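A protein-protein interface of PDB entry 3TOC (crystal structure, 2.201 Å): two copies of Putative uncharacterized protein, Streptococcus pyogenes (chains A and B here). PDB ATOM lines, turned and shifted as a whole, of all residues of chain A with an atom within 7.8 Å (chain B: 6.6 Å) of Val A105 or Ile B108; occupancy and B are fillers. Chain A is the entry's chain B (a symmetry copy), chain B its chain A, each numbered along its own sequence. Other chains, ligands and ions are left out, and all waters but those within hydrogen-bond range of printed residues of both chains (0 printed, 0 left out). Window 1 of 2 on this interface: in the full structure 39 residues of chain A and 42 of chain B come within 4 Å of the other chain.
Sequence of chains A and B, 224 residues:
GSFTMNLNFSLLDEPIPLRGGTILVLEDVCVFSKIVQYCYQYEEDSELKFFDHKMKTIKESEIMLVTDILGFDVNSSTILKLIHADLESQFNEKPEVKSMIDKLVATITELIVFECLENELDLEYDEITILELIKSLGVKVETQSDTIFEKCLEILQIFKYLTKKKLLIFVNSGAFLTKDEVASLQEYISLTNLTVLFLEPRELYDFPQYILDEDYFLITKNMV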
ATOM      1  N   PHE A  91      21.377  28.830 -37.852  1.00  0.00           N
ATOM      2  CA  PHE A  91      21.352  27.723 -36.920  1.00  0.00           C
ATOM      3  C   PHE A  91      20.137  26.848 -37.145  1.00  0.00           C
ATOM      4  O   PHE A  91      20.236  25.625 -37.154  1.00  0.00           O
ATOM      5  CB  PHE A  91      21.335  28.253 -35.505  1.00  0.00           C
ATOM      6  CG  PHE A  91      22.676  28.611 -34.994  1.00  0.00           C
ATOM      7  CD1 PHE A  91      23.658  27.647 -34.878  1.00  0.00           C
ATOM      8  CD2 PHE A  91      22.964  29.893 -34.618  1.00  0.00           C
ATOM      9  CE1 PHE A  91      24.912  27.968 -34.397  1.00  0.00           C
ATOM     10  CE2 PHE A  91      24.211  30.219 -34.137  1.00  0.00           C
ATOM     11  CZ  PHE A  91      25.185  29.251 -34.026  1.00  0.00           C
ATOM     12  N   LYS A  98      22.447  23.078 -34.335  1.00  0.00           N
ATOM     13  CA  LYS A  98      21.437  23.529 -33.401  1.00  0.00           C
ATOM     14  C   LYS A  98      21.452  22.580 -32.205  1.00  0.00           C
ATOM     15  O   LYS A  98      21.584  22.998 -31.055  1.00  0.00           O
ATOM     16  CB  LYS A  98      20.071  23.516 -34.091  1.00  0.00           C
ATOM     17  CG  LYS A  98      18.901  23.908 -33.224  1.00  0.00           C
ATOM     18  CD  LYS A  98      18.882  25.394 -32.938  1.00  0.00           C
ATOM     19  CE  LYS A  98      17.666  25.764 -32.088  1.00  0.00           C
ATOM     20  NZ  LYS A  98      16.394  25.305 -32.747  1.00  0.00           N
ATOM     21  N   SER A  99      21.338  21.290 -32.492  1.00  0.00           N
ATOM     22  CA  SER A  99      21.366  20.286 -31.444  1.00  0.00           C
ATOM     23  C   SER A  99      22.562  20.506 -30.512  1.00  0.00           C
ATOM     24  O   SER A  99      22.426  20.459 -29.291  1.00  0.00           O
ATOM     25  CB  SER A  99      21.414  18.892 -32.048  1.00  0.00           C
ATOM     26  OG  SER A  99      21.208  17.923 -31.042  1.00  0.00           O
ATOM     27  N   MET A 100      23.731  20.761 -31.086  1.00  0.00           N
ATOM     28  CA  MET A 100      24.929  20.958 -30.277  1.00  0.00           C
ATOM     29  C   MET A 100      24.777  22.197 -29.383  1.00  0.00           C
ATOM     30  O   MET A 100      25.073  22.166 -28.173  1.00  0.00           O
ATOM     31  CB  MET A 100      26.172  21.070 -31.164  1.00  0.00           C
ATOM     32  CG  MET A 100      27.462  21.143 -30.380  1.00  0.00           C
ATOM     33  SD  MET A 100      27.778  19.490 -29.357  1.00  0.00           S
ATOM     34  CE  MET A 100      29.335  20.031 -28.316  1.00  0.00           C
ATOM     35  N   ILE A 101      24.313  23.290 -29.986  1.00  0.00           N
ATOM     36  CA  ILE A 101      24.032  24.506 -29.239  1.00  0.00           C
ATOM     37  C   ILE A 101      23.094  24.197 -28.051  1.00  0.00           C
ATOM     38  O   ILE A 101      23.370  24.571 -26.906  1.00  0.00           O
ATOM     39  CB  ILE A 101      23.410  25.610 -30.142  1.00  0.00           C
ATOM     40  CG1 ILE A 101      24.465  26.236 -31.039  1.00  0.00           C
ATOM     41  CG2 ILE A 101      22.839  26.728 -29.282  1.00  0.00           C
ATOM     42  CD1 ILE A 101      25.438  27.107 -30.267  1.00  0.00           C
ATOM     43  N   ASP A 102      21.988  23.509 -28.317  1.00  0.00           N
ATOM     44  CA  ASP A 102      21.056  23.167 -27.248  1.00  0.00           C
ATOM     45  C   ASP A 102      21.731  22.442 -26.076  1.00  0.00           C
ATOM     46  O   ASP A 102      21.511  22.813 -24.908  1.00  0.00           O
ATOM     47  CB  ASP A 102      19.898  22.332 -27.801  1.00  0.00           C
ATOM     48  CG  ASP A 102      19.054  23.101 -28.810  1.00  0.00           C
ATOM     49  OD1 ASP A 102      19.119  24.355 -28.802  1.00  0.00           O
ATOM     50  OD2 ASP A 102      18.319  22.457 -29.595  1.00  0.00           O
ATOM     51  N   LYS A 103      22.551  21.421 -26.374  1.00  0.00           N
ATOM     52  CA  LYS A 103      23.213  20.645 -25.315  1.00  0.00           C
ATOM     53  C   LYS A 103      24.109  21.548 -24.472  1.00  0.00           C
ATOM     54  O   LYS A 103      24.080  21.484 -23.246  1.00  0.00           O
ATOM     55  CB  LYS A 103      24.009  19.466 -25.891  1.00  0.00           C
ATOM     56  CG  LYS A 103      23.109  18.425 -26.563  1.00  0.00           C
ATOM     57  CD  LYS A 103      23.832  17.432 -27.479  1.00  0.00           C
ATOM     58  CE  LYS A 103      22.788  16.555 -28.181  1.00  0.00           C
ATOM     59  NZ  LYS A 103      23.369  15.596 -29.163  1.00  0.00           N
ATOM     60  N   LEU A 104      24.892  22.400 -25.132  1.00  0.00           N
ATOM     61  CA  LEU A 104      25.824  23.281 -24.420  1.00  0.00           C
ATOM     62  C   LEU A 104      25.088  24.283 -23.518  1.00  0.00           C
ATOM     63  O   LEU A 104      25.540  24.598 -22.403  1.00  0.00           O
ATOM     64  CB  LEU A 104      26.685  24.053 -25.420  1.00  0.00           C
ATOM     65  CG  LEU A 104      27.681  23.279 -26.284  1.00  0.00           C
ATOM     66  CD1 LEU A 104      28.100  24.109 -27.498  1.00  0.00           C
ATOM     67  CD2 LEU A 104      28.885  22.873 -25.462  1.00  0.00           C
ATOM     68  N   VAL A 105      23.972  24.811 -24.018  1.00  0.00           N
ATOM     69  CA  VAL A 105      23.198  25.787 -23.252  1.00  0.00           C
ATOM     70  C   VAL A 105      22.452  25.111 -22.096  1.00  0.00           C
ATOM     71  O   VAL A 105      22.389  25.653 -21.002  1.00  0.00           O
ATOM     72  CB  VAL A 105      22.210  26.587 -24.118  1.00  0.00           C
ATOM     73  CG1 VAL A 105      21.312  27.449 -23.227  1.00  0.00           C
ATOM     74  CG2 VAL A 105      22.940  27.452 -25.132  1.00  0.00           C
ATOM     75  N   ALA A 106      21.903  23.924 -22.329  1.00  0.00           N
ATOM     76  CA  ALA A 106      21.270  23.201 -21.233  1.00  0.00           C
ATOM     77  C   ALA A 106      22.280  22.906 -20.112  1.00  0.00           C
ATOM     78  O   ALA A 106      21.930  22.894 -18.922  1.00  0.00           O
ATOM     79  CB  ALA A 106      20.609  21.934 -21.717  1.00  0.00           C
ATOM     80  N   THR A 107      23.540  22.702 -20.473  1.00  0.00           N
ATOM     81  CA  THR A 107      24.523  22.342 -19.455  1.00  0.00           C
ATOM     82  C   THR A 107      24.991  23.554 -18.676  1.00  0.00           C
ATOM     83  O   THR A 107      25.080  23.534 -17.445  1.00  0.00           O
ATOM     84  CB  THR A 107      25.738  21.609 -20.067  1.00  0.00           C
ATOM     85  OG1 THR A 107      25.289  20.403 -20.691  1.00  0.00           O
ATOM     86  CG2 THR A 107      26.757  21.275 -18.996  1.00  0.00           C
ATOM     87  N   ILE A 108      25.321  24.608 -19.403  1.00  0.00           N
ATOM     88  CA  ILE A 108      25.681  25.862 -18.768  1.00  0.00           C
ATOM     89  C   ILE A 108      24.530  26.322 -17.872  1.00  0.00           C
ATOM     90  O   ILE A 108      24.746  26.860 -16.785  1.00  0.00           O
ATOM     91  CB  ILE A 108      25.945  26.918 -19.829  1.00  0.00           C
ATOM     92  CG1 ILE A 108      27.182  26.540 -20.632  1.00  0.00           C
ATOM     93  CG2 ILE A 108      26.072  28.294 -19.214  1.00  0.00           C
ATOM     94  CD1 ILE A 108      27.525  27.568 -21.681  1.00  0.00           C
ATOM     95  N   THR A 109      23.304  26.106 -18.338  1.00  0.00           N
ATOM     96  CA  THR A 109      22.120  26.444 -17.558  1.00  0.00           C
ATOM     97  C   THR A 109      22.071  25.670 -16.241  1.00  0.00           C
ATOM     98  O   THR A 109      21.961  26.271 -15.164  1.00  0.00           O
ATOM     99  CB  THR A 109      20.830  26.210 -18.345  1.00  0.00           C
ATOM    100  OG1 THR A 109      20.783  27.122 -19.455  1.00  0.00           O
ATOM    101  CG2 THR A 109      19.620  26.468 -17.450  1.00  0.00           C
ATOM    102  N   GLU A 110      22.197  24.347 -16.304  1.00  0.00           N
ATOM    103  CA  GLU A 110      22.176  23.587 -15.057  1.00  0.00           C
ATOM    104  C   GLU A 110      23.272  24.090 -14.132  1.00  0.00           C
ATOM    105  O   GLU A 110      23.032  24.299 -12.956  1.00  0.00           O
ATOM    106  CB  GLU A 110      22.277  22.078 -15.274  1.00  0.00           C
ATOM    107  CG  GLU A 110      20.957  21.415 -15.639  1.00  0.00           C
ATOM    108  CD  GLU A 110      20.917  19.937 -15.285  1.00  0.00           C
ATOM    109  OE1 GLU A 110      19.939  19.246 -15.650  1.00  0.00           O
ATOM    110  OE2 GLU A 110      21.863  19.466 -14.634  1.00  0.00           O
ATOM    111  N   LEU A 111      24.469  24.304 -14.664  1.00  0.00           N
ATOM    112  CA  LEU A 111      25.575  24.726 -13.811  1.00  0.00           C
ATOM    113  C   LEU A 111      25.265  26.029 -13.118  1.00  0.00           C
ATOM    114  O   LEU A 111      25.665  26.220 -11.975  1.00  0.00           O
ATOM    115  CB  LEU A 111      26.871  24.836 -14.600  1.00  0.00           C
ATOM    116  CG  LEU A 111      27.233  23.493 -15.231  1.00  0.00           C
ATOM    117  CD1 LEU A 111      28.433  23.621 -16.184  1.00  0.00           C
ATOM    118  CD2 LEU A 111      27.478  22.440 -14.129  1.00  0.00           C
ATOM    119  N   ILE A 112      24.574  26.935 -13.820  1.00  0.00           N
ATOM    120  CA  ILE A 112      24.165  28.213 -13.234  1.00  0.00           C
ATOM    121  C   ILE A 112      23.042  28.028 -12.224  1.00  0.00           C
ATOM    122  O   ILE A 112      23.095  28.559 -11.104  1.00  0.00           O
ATOM    123  CB  ILE A 112      23.728  29.248 -14.294  1.00  0.00           C
ATOM    124  CG1 ILE A 112      24.915  29.623 -15.182  1.00  0.00           C
ATOM    125  CG2 ILE A 112      23.203  30.505 -13.617  1.00  0.00           C
ATOM    126  CD1 ILE A 112      24.551  30.512 -16.351  1.00  0.00           C
ATOM    127  N   GLU A 127      15.220  31.106 -19.516  1.00  0.00           N
ATOM    128  CA  GLU A 127      16.069  30.254 -20.339  1.00  0.00           C
ATOM    129  C   GLU A 127      17.004  31.109 -21.133  1.00  0.00           C
ATOM    130  O   GLU A 127      16.699  32.248 -21.390  1.00  0.00           O
ATOM    131  CB  GLU A 127      15.207  29.491 -21.328  1.00  0.00           C
ATOM    132  CG  GLU A 127      14.511  30.428 -22.275  1.00  0.00           C
ATOM    133  CD  GLU A 127      13.704  29.696 -23.315  1.00  0.00           C
ATOM    134  OE1 GLU A 127      13.691  28.445 -23.277  1.00  0.00           O
ATOM    135  OE2 GLU A 127      13.083  30.373 -24.169  1.00  0.00           O
ATOM    136  N   ILE A 128      18.132  30.554 -21.546  1.00  0.00           N
ATOM    137  CA  ILE A 128      19.040  31.275 -22.425  1.00  0.00           C
ATOM    138  C   ILE A 128      18.719  30.925 -23.875  1.00  0.00           C
ATOM    139  O   ILE A 128      18.616  29.752 -24.223  1.00  0.00           O
ATOM    140  CB  ILE A 128      20.481  30.922 -22.084  1.00  0.00           C
ATOM    141  CG1 ILE A 128      20.771  31.313 -20.638  1.00  0.00           C
ATOM    142  CG2 ILE A 128      21.456  31.609 -23.024  1.00  0.00           C
ATOM    143  CD1 ILE A 128      22.165  30.900 -20.155  1.00  0.00           C
ATOM    144  N   THR A 129      18.518  31.936 -24.717  1.00  0.00           N
ATOM    145  CA  THR A 129      18.160  31.685 -26.111  1.00  0.00           C
ATOM    146  C   THR A 129      19.355  31.939 -27.041  1.00  0.00           C
ATOM    147  O   THR A 129      20.330  32.578 -26.631  1.00  0.00           O
ATOM    148  CB  THR A 129      16.972  32.550 -26.542  1.00  0.00           C
ATOM    149  OG1 THR A 129      17.415  33.903 -26.732  1.00  0.00           O
ATOM    150  CG2 THR A 129      15.870  32.491 -25.472  1.00  0.00           C
ATOM    151  N   ILE A 130      19.296  31.442 -28.280  1.00  0.00           N
ATOM    152  CA  ILE A 130      20.413  31.643 -29.206  1.00  0.00           C
ATOM    153  C   ILE A 130      20.555  33.118 -29.534  1.00  0.00           C
ATOM    154  O   ILE A 130      21.644  33.629 -29.749  1.00  0.00           O
ATOM    155  CB  ILE A 130      20.254  30.877 -30.529  1.00  0.00           C
ATOM    156  CG1 ILE A 130      20.019  29.400 -30.269  1.00  0.00           C
ATOM    157  CG2 ILE A 130      21.524  30.998 -31.360  1.00  0.00           C
ATOM    158  CD1 ILE A 130      20.033  28.550 -31.527  1.00  0.00           C
ATOM    159  N   GLU A 132      19.946  35.565 -27.578  1.00  0.00           N
ATOM    160  CA  GLU A 132      20.642  36.127 -26.420  1.00  0.00           C
ATOM    161  C   GLU A 132      22.151  35.878 -26.401  1.00  0.00           C
ATOM    162  O   GLU A 132      22.916  36.745 -25.991  1.00  0.00           O
ATOM    163  CB  GLU A 132      20.011  35.616 -25.120  1.00  0.00           C
ATOM    164  CG  GLU A 132      18.622  36.183 -24.892  1.00  0.00           C
ATOM    165  CD  GLU A 132      17.949  35.587 -23.686  1.00  0.00           C
ATOM    166  OE1 GLU A 132      18.213  34.404 -23.378  1.00  0.00           O
ATOM    167  OE2 GLU A 132      17.174  36.319 -23.036  1.00  0.00           O
ATOM    168  N   LEU A 133      22.573  34.683 -26.808  1.00  0.00           N
ATOM    169  CA  LEU A 133      23.995  34.414 -27.005  1.00  0.00           C
ATOM    170  C   LEU A 133      24.571  35.291 -28.122  1.00  0.00           C
ATOM    171  O   LEU A 133      25.600  35.935 -27.937  1.00  0.00           O
ATOM    172  CB  LEU A 133      24.205  32.946 -27.328  1.00  0.00           C
ATOM    173  CG  LEU A 133      23.789  32.037 -26.167  1.00  0.00           C
ATOM    174  CD1 LEU A 133      23.760  30.625 -26.648  1.00  0.00           C
ATOM    175  CD2 LEU A 133      24.725  32.204 -24.973  1.00  0.00           C
ATOM    176  N   ILE A 134      23.898  35.327 -29.268  1.00  0.00           N
ATOM    177  CA  ILE A 134      24.338  36.179 -30.373  1.00  0.00           C
ATOM    178  C   ILE A 134      24.463  37.630 -29.921  1.00  0.00           C
ATOM    179  O   ILE A 134      25.481  38.268 -30.167  1.00  0.00           O
ATOM    180  CB  ILE A 134      23.417  36.068 -31.603  1.00  0.00           C
ATOM    181  CG1 ILE A 134      23.447  34.645 -32.153  1.00  0.00           C
ATOM    182  CG2 ILE A 134      23.858  37.039 -32.680  1.00  0.00           C
ATOM    183  CD1 ILE A 134      22.365  34.354 -33.152  1.00  0.00           C
ATOM    184  N   LEU A 137      27.436  38.106 -27.360  1.00  0.00           N
ATOM    185  CA  LEU A 137      28.738  38.041 -28.007  1.00  0.00           C
ATOM    186  C   LEU A 137      29.087  39.386 -28.669  1.00  0.00           C
ATOM    187  O   LEU A 137      30.243  39.647 -28.981  1.00  0.00           O
ATOM    188  CB  LEU A 137      28.783  36.883 -29.030  1.00  0.00           C
ATOM    189  CG  LEU A 137      30.068  36.649 -29.857  1.00  0.00           C
ATOM    190  CD1 LEU A 137      31.295  36.420 -28.969  1.00  0.00           C
ATOM    191  CD2 LEU A 137      29.912  35.501 -30.833  1.00  0.00           C
ATOM    192  N   LYS B 103      34.995  26.698 -21.181  1.00  0.00           N
ATOM    193  CA  LYS B 103      35.218  25.838 -22.331  1.00  0.00           C
ATOM    194  C   LYS B 103      33.912  25.624 -23.101  1.00  0.00           C
ATOM    195  O   LYS B 103      33.900  25.561 -24.334  1.00  0.00           O
ATOM    196  CB  LYS B 103      35.845  24.510 -21.890  1.00  0.00           C
ATOM    197  CG  LYS B 103      35.689  23.387 -22.883  1.00  0.00           C
ATOM    198  CD  LYS B 103      36.660  23.499 -24.054  1.00  0.00           C
ATOM    199  CE  LYS B 103      36.558  22.265 -24.954  1.00  0.00           C
ATOM    200  NZ  LYS B 103      36.482  20.997 -24.148  1.00  0.00           N
ATOM    201  N   LEU B 104      32.807  25.527 -22.378  1.00  0.00           N
ATOM    202  CA  LEU B 104      31.514  25.365 -23.025  1.00  0.00           C
ATOM    203  C   LEU B 104      31.166  26.632 -23.799  1.00  0.00           C
ATOM    204  O   LEU B 104      30.674  26.571 -24.918  1.00  0.00           O
ATOM    205  CB  LEU B 104      30.433  25.048 -21.992  1.00  0.00           C
ATOM    206  CG  LEU B 104      30.598  23.691 -21.287  1.00  0.00           C
ATOM    207  CD1 LEU B 104      29.493  23.499 -20.257  1.00  0.00           C
ATOM    208  CD2 LEU B 104      30.574  22.561 -22.294  1.00  0.00           C
ATOM    209  N   VAL B 105      31.443  27.780 -23.201  1.00  0.00           N
ATOM    210  CA  VAL B 105      31.167  29.057 -23.845  1.00  0.00           C
ATOM    211  C   VAL B 105      32.095  29.295 -25.040  1.00  0.00           C
ATOM    212  O   VAL B 105      31.667  29.855 -26.046  1.00  0.00           O
ATOM    213  CB  VAL B 105      31.303  30.218 -22.862  1.00  0.00           C
ATOM    214  CG1 VAL B 105      31.385  31.550 -23.607  1.00  0.00           C
ATOM    215  CG2 VAL B 105      30.147  30.192 -21.873  1.00  0.00           C
ATOM    216  N   ALA B 106      33.354  28.860 -24.949  1.00  0.00           N
ATOM    217  CA  ALA B 106      34.234  28.966 -26.112  1.00  0.00           C
ATOM    218  C   ALA B 106      33.641  28.155 -27.264  1.00  0.00           C
ATOM    219  O   ALA B 106      33.618  28.607 -28.419  1.00  0.00           O
ATOM    220  CB  ALA B 106      35.647  28.512 -25.787  1.00  0.00           C
ATOM    221  N   THR B 107      33.140  26.962 -26.955  1.00  0.00           N
ATOM    222  CA  THR B 107      32.581  26.117 -28.011  1.00  0.00           C
ATOM    223  C   THR B 107      31.382  26.824 -28.610  1.00  0.00           C
ATOM    224  O   THR B 107      31.215  26.846 -29.820  1.00  0.00           O
ATOM    225  CB  THR B 107      32.164  24.734 -27.490  1.00  0.00           C
ATOM    226  OG1 THR B 107      33.296  24.096 -26.902  1.00  0.00           O
ATOM    227  CG2 THR B 107      31.629  23.855 -28.615  1.00  0.00           C
ATOM    228  N   ILE B 108      30.548  27.410 -27.753  1.00  0.00           N
ATOM    229  CA  ILE B 108      29.404  28.143 -28.247  1.00  0.00           C
ATOM    230  C   ILE B 108      29.881  29.284 -29.132  1.00  0.00           C
ATOM    231  O   ILE B 108      29.432  29.436 -30.270  1.00  0.00           O
ATOM    232  CB  ILE B 108      28.554  28.717 -27.115  1.00  0.00           C
ATOM    233  CG1 ILE B 108      27.759  27.602 -26.418  1.00  0.00           C
ATOM    234  CG2 ILE B 108      27.602  29.774 -27.670  1.00  0.00           C
ATOM    235  CD1 ILE B 108      26.872  28.099 -25.305  1.00  0.00           C
ATOM    236  N   THR B 109      30.813  30.069 -28.598  1.00  0.00           N
ATOM    237  CA  THR B 109      31.390  31.192 -29.318  1.00  0.00           C
ATOM    238  C   THR B 109      31.903  30.751 -30.661  1.00  0.00           C
ATOM    239  O   THR B 109      31.705  31.416 -31.666  1.00  0.00           O
ATOM    240  CB  THR B 109      32.534  31.783 -28.532  1.00  0.00           C
ATOM    241  OG1 THR B 109      32.016  32.231 -27.279  1.00  0.00           O
ATOM    242  CG2 THR B 109      33.130  32.964 -29.284  1.00  0.00           C
ATOM    243  N   GLU B 110      32.540  29.591 -30.674  1.00  0.00           N
ATOM    244  CA  GLU B 110      33.127  29.071 -31.890  1.00  0.00           C
ATOM    245  C   GLU B 110      32.067  28.746 -32.928  1.00  0.00           C
ATOM    246  O   GLU B 110      32.234  29.036 -34.099  1.00  0.00           O
ATOM    247  CB  GLU B 110      33.938  27.819 -31.565  1.00  0.00           C
ATOM    248  CG  GLU B 110      34.452  27.083 -32.756  1.00  0.00           C
ATOM    249  CD  GLU B 110      35.184  25.820 -32.350  1.00  0.00           C
ATOM    250  OE1 GLU B 110      35.183  25.507 -31.134  1.00  0.00           O
ATOM    251  OE2 GLU B 110      35.754  25.146 -33.242  1.00  0.00           O
ATOM    252  N   LEU B 111      30.972  28.131 -32.508  1.00  0.00           N
ATOM    253  CA  LEU B 111      29.915  27.832 -33.461  1.00  0.00           C
ATOM    254  C   LEU B 111      29.293  29.116 -33.988  1.00  0.00           C
ATOM    255  O   LEU B 111      28.914  29.178 -35.147  1.00  0.00           O
ATOM    256  CB  LEU B 111      28.839  26.926 -32.846  1.00  0.00           C
ATOM    257  CG  LEU B 111      29.317  25.522 -32.449  1.00  0.00           C
ATOM    258  CD1 LEU B 111      28.252  24.789 -31.644  1.00  0.00           C
ATOM    259  CD2 LEU B 111      29.760  24.710 -33.675  1.00  0.00           C
ATOM    260  N   ILE B 112      29.168  30.134 -33.140  1.00  0.00           N
ATOM    261  CA  ILE B 112      28.548  31.379 -33.584  1.00  0.00           C
ATOM    262  C   ILE B 112      29.486  32.120 -34.526  1.00  0.00           C
ATOM    263  O   ILE B 112      29.061  32.597 -35.568  1.00  0.00           O
ATOM    264  CB  ILE B 112      28.122  32.285 -32.424  1.00  0.00           C
ATOM    265  CG1 ILE B 112      27.015  31.601 -31.616  1.00  0.00           C
ATOM    266  CG2 ILE B 112      27.579  33.628 -32.951  1.00  0.00           C
ATOM    267  CD1 ILE B 112      26.565  32.379 -30.428  1.00  0.00           C
ATOM    268  N   VAL B 113      30.762  32.196 -34.167  1.00  0.00           N
ATOM    269  CA  VAL B 113      31.716  32.875 -35.009  1.00  0.00           C
ATOM    270  C   VAL B 113      31.765  32.199 -36.383  1.00  0.00           C
ATOM    271  O   VAL B 113      31.950  32.852 -37.415  1.00  0.00           O
ATOM    272  CB  VAL B 113      33.109  32.880 -34.390  1.00  0.00           C
ATOM    273  CG1 VAL B 113      34.153  33.312 -35.439  1.00  0.00           C
ATOM    274  CG2 VAL B 113      33.139  33.799 -33.182  1.00  0.00           C
ATOM    275  N   ILE B 128      31.428  36.189 -24.900  1.00  0.00           N
ATOM    276  CA  ILE B 128      30.276  35.967 -24.046  1.00  0.00           C
ATOM    277  C   ILE B 128      30.777  35.759 -22.635  1.00  0.00           C
ATOM    278  O   ILE B 128      31.656  34.934 -22.426  1.00  0.00           O
ATOM    279  CB  ILE B 128      29.535  34.718 -24.475  1.00  0.00           C
ATOM    280  CG1 ILE B 128      28.959  34.898 -25.884  1.00  0.00           C
ATOM    281  CG2 ILE B 128      28.461  34.353 -23.451  1.00  0.00           C
ATOM    282  CD1 ILE B 128      28.324  33.629 -26.458  1.00  0.00           C
ATOM    283  N   LEU B 133      25.552  35.500 -19.347  1.00  0.00           N
ATOM    284  CA  LEU B 133      24.750  34.292 -19.315  1.00  0.00           C
ATOM    285  C   LEU B 133      23.738  34.350 -18.180  1.00  0.00           C
ATOM    286  O   LEU B 133      22.567  34.033 -18.347  1.00  0.00           O
ATOM    287  CB  LEU B 133      25.654  33.076 -19.130  1.00  0.00           C
ATOM    288  CG  LEU B 133      26.562  32.862 -20.352  1.00  0.00           C
ATOM    289  CD1 LEU B 133      27.447  31.628 -20.151  1.00  0.00           C
ATOM    290  CD2 LEU B 133      25.753  32.734 -21.637  1.00  0.00           C
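OG1 of Thr B107 is in hydrogen-bond range of O of Lys B103 (3.0 Å). O of Val B105 sits at hydrogen-bond distance from OG1 of Thr B109. OG1 of Thr A107 lies within hydrogen-bond range of O of Lys A103. O of Val A105 lies within hydrogen-bond range of OG1 of Thr A109 (2.7 Å).
Among the printed residues, pairs that only touch across the chains: Leu A133 with Leu B133 (3.5 Å), Leu A104 with Leu B104 (3.6 Å), Ile A128 with Leu B133 (3.6 Å), Leu A137 with Ile B112 (3.7 Å), Leu A104 with Ile B108 (3.7 Å), Leu A104 with Thr B107 (3.7 Å), Ile A108 with Val B105 (3.7 Å), Ile A108 with Ile B108 (3.7 Å), Leu A137 with Ile B128 (3.7 Å), Ile A108 with Leu B133 (3.7 Å), Thr A107 with Leu B104 (3.7 Å), Ile A108 with Leu B104 (3.8 Å), Phe A91 with Ile B112 (3.8 Å), Leu A133 with Ile B128 (3.9 Å), Phe A91 with Leu B111 (3.9 Å), Ile A101 with Leu B111 (3.9 Å), Leu A137 with Thr B109 (3.9 Å), Leu A133 with Ile B112 (3.9 Å), Ile A112 with Leu B133 (3.9 Å), Met A100 with Leu B111 (3.9 Å) and Val A105 with Ile B108 (3.99 Å).
Of the printed residues of chain B, Val A105 touches Ile B108. Of the printed residues of chain B, Ile A128 touches Leu B133. Printed residues of chain B within 4 Å of Leu A133: Ile B112, Ile B128 and Leu B133. Printed residues of chain A within 4 Å of Ile B108: Leu A104 (3.7 Å), Val A105 (3.99 Å) and Ile A108 (3.7 Å). Val B113 touches none of the printed residues of chain A. The nearest printed residue of chain A that does not touch Ile B108 is Leu A133 (4.1 Å).
Hydrophobic or aromatic side chains of chain A that line the printed part of chain B: Phe A91, Met A100, Ile A101, Leu A104, Val A105, Ile A108, Ile A112, Ile A128, Leu A133 and Leu A137. Among the printed residues, no Asp or Glu carboxylate lies within 4 Å of a Lys or Arg side-chain nitrogen of the other chain.
Leu A104 touches Thr B107, and with the chains exchanged Thr A107 touches Leu B104. Val A105 touches Ile B108, and with the chains exchanged Ile A108 touches Val B105. Ile A108 touches Leu B133, but with the chains exchanged Leu A133 does not touch Ile B108 (4.1 Å). Ile A112 touches Leu B133, and with the chains exchanged Leu A133 touches Ile B112. Of the 21 pairs that touch across the chains among the printed residues, 13 have their exchanged pair printed and touching as well.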
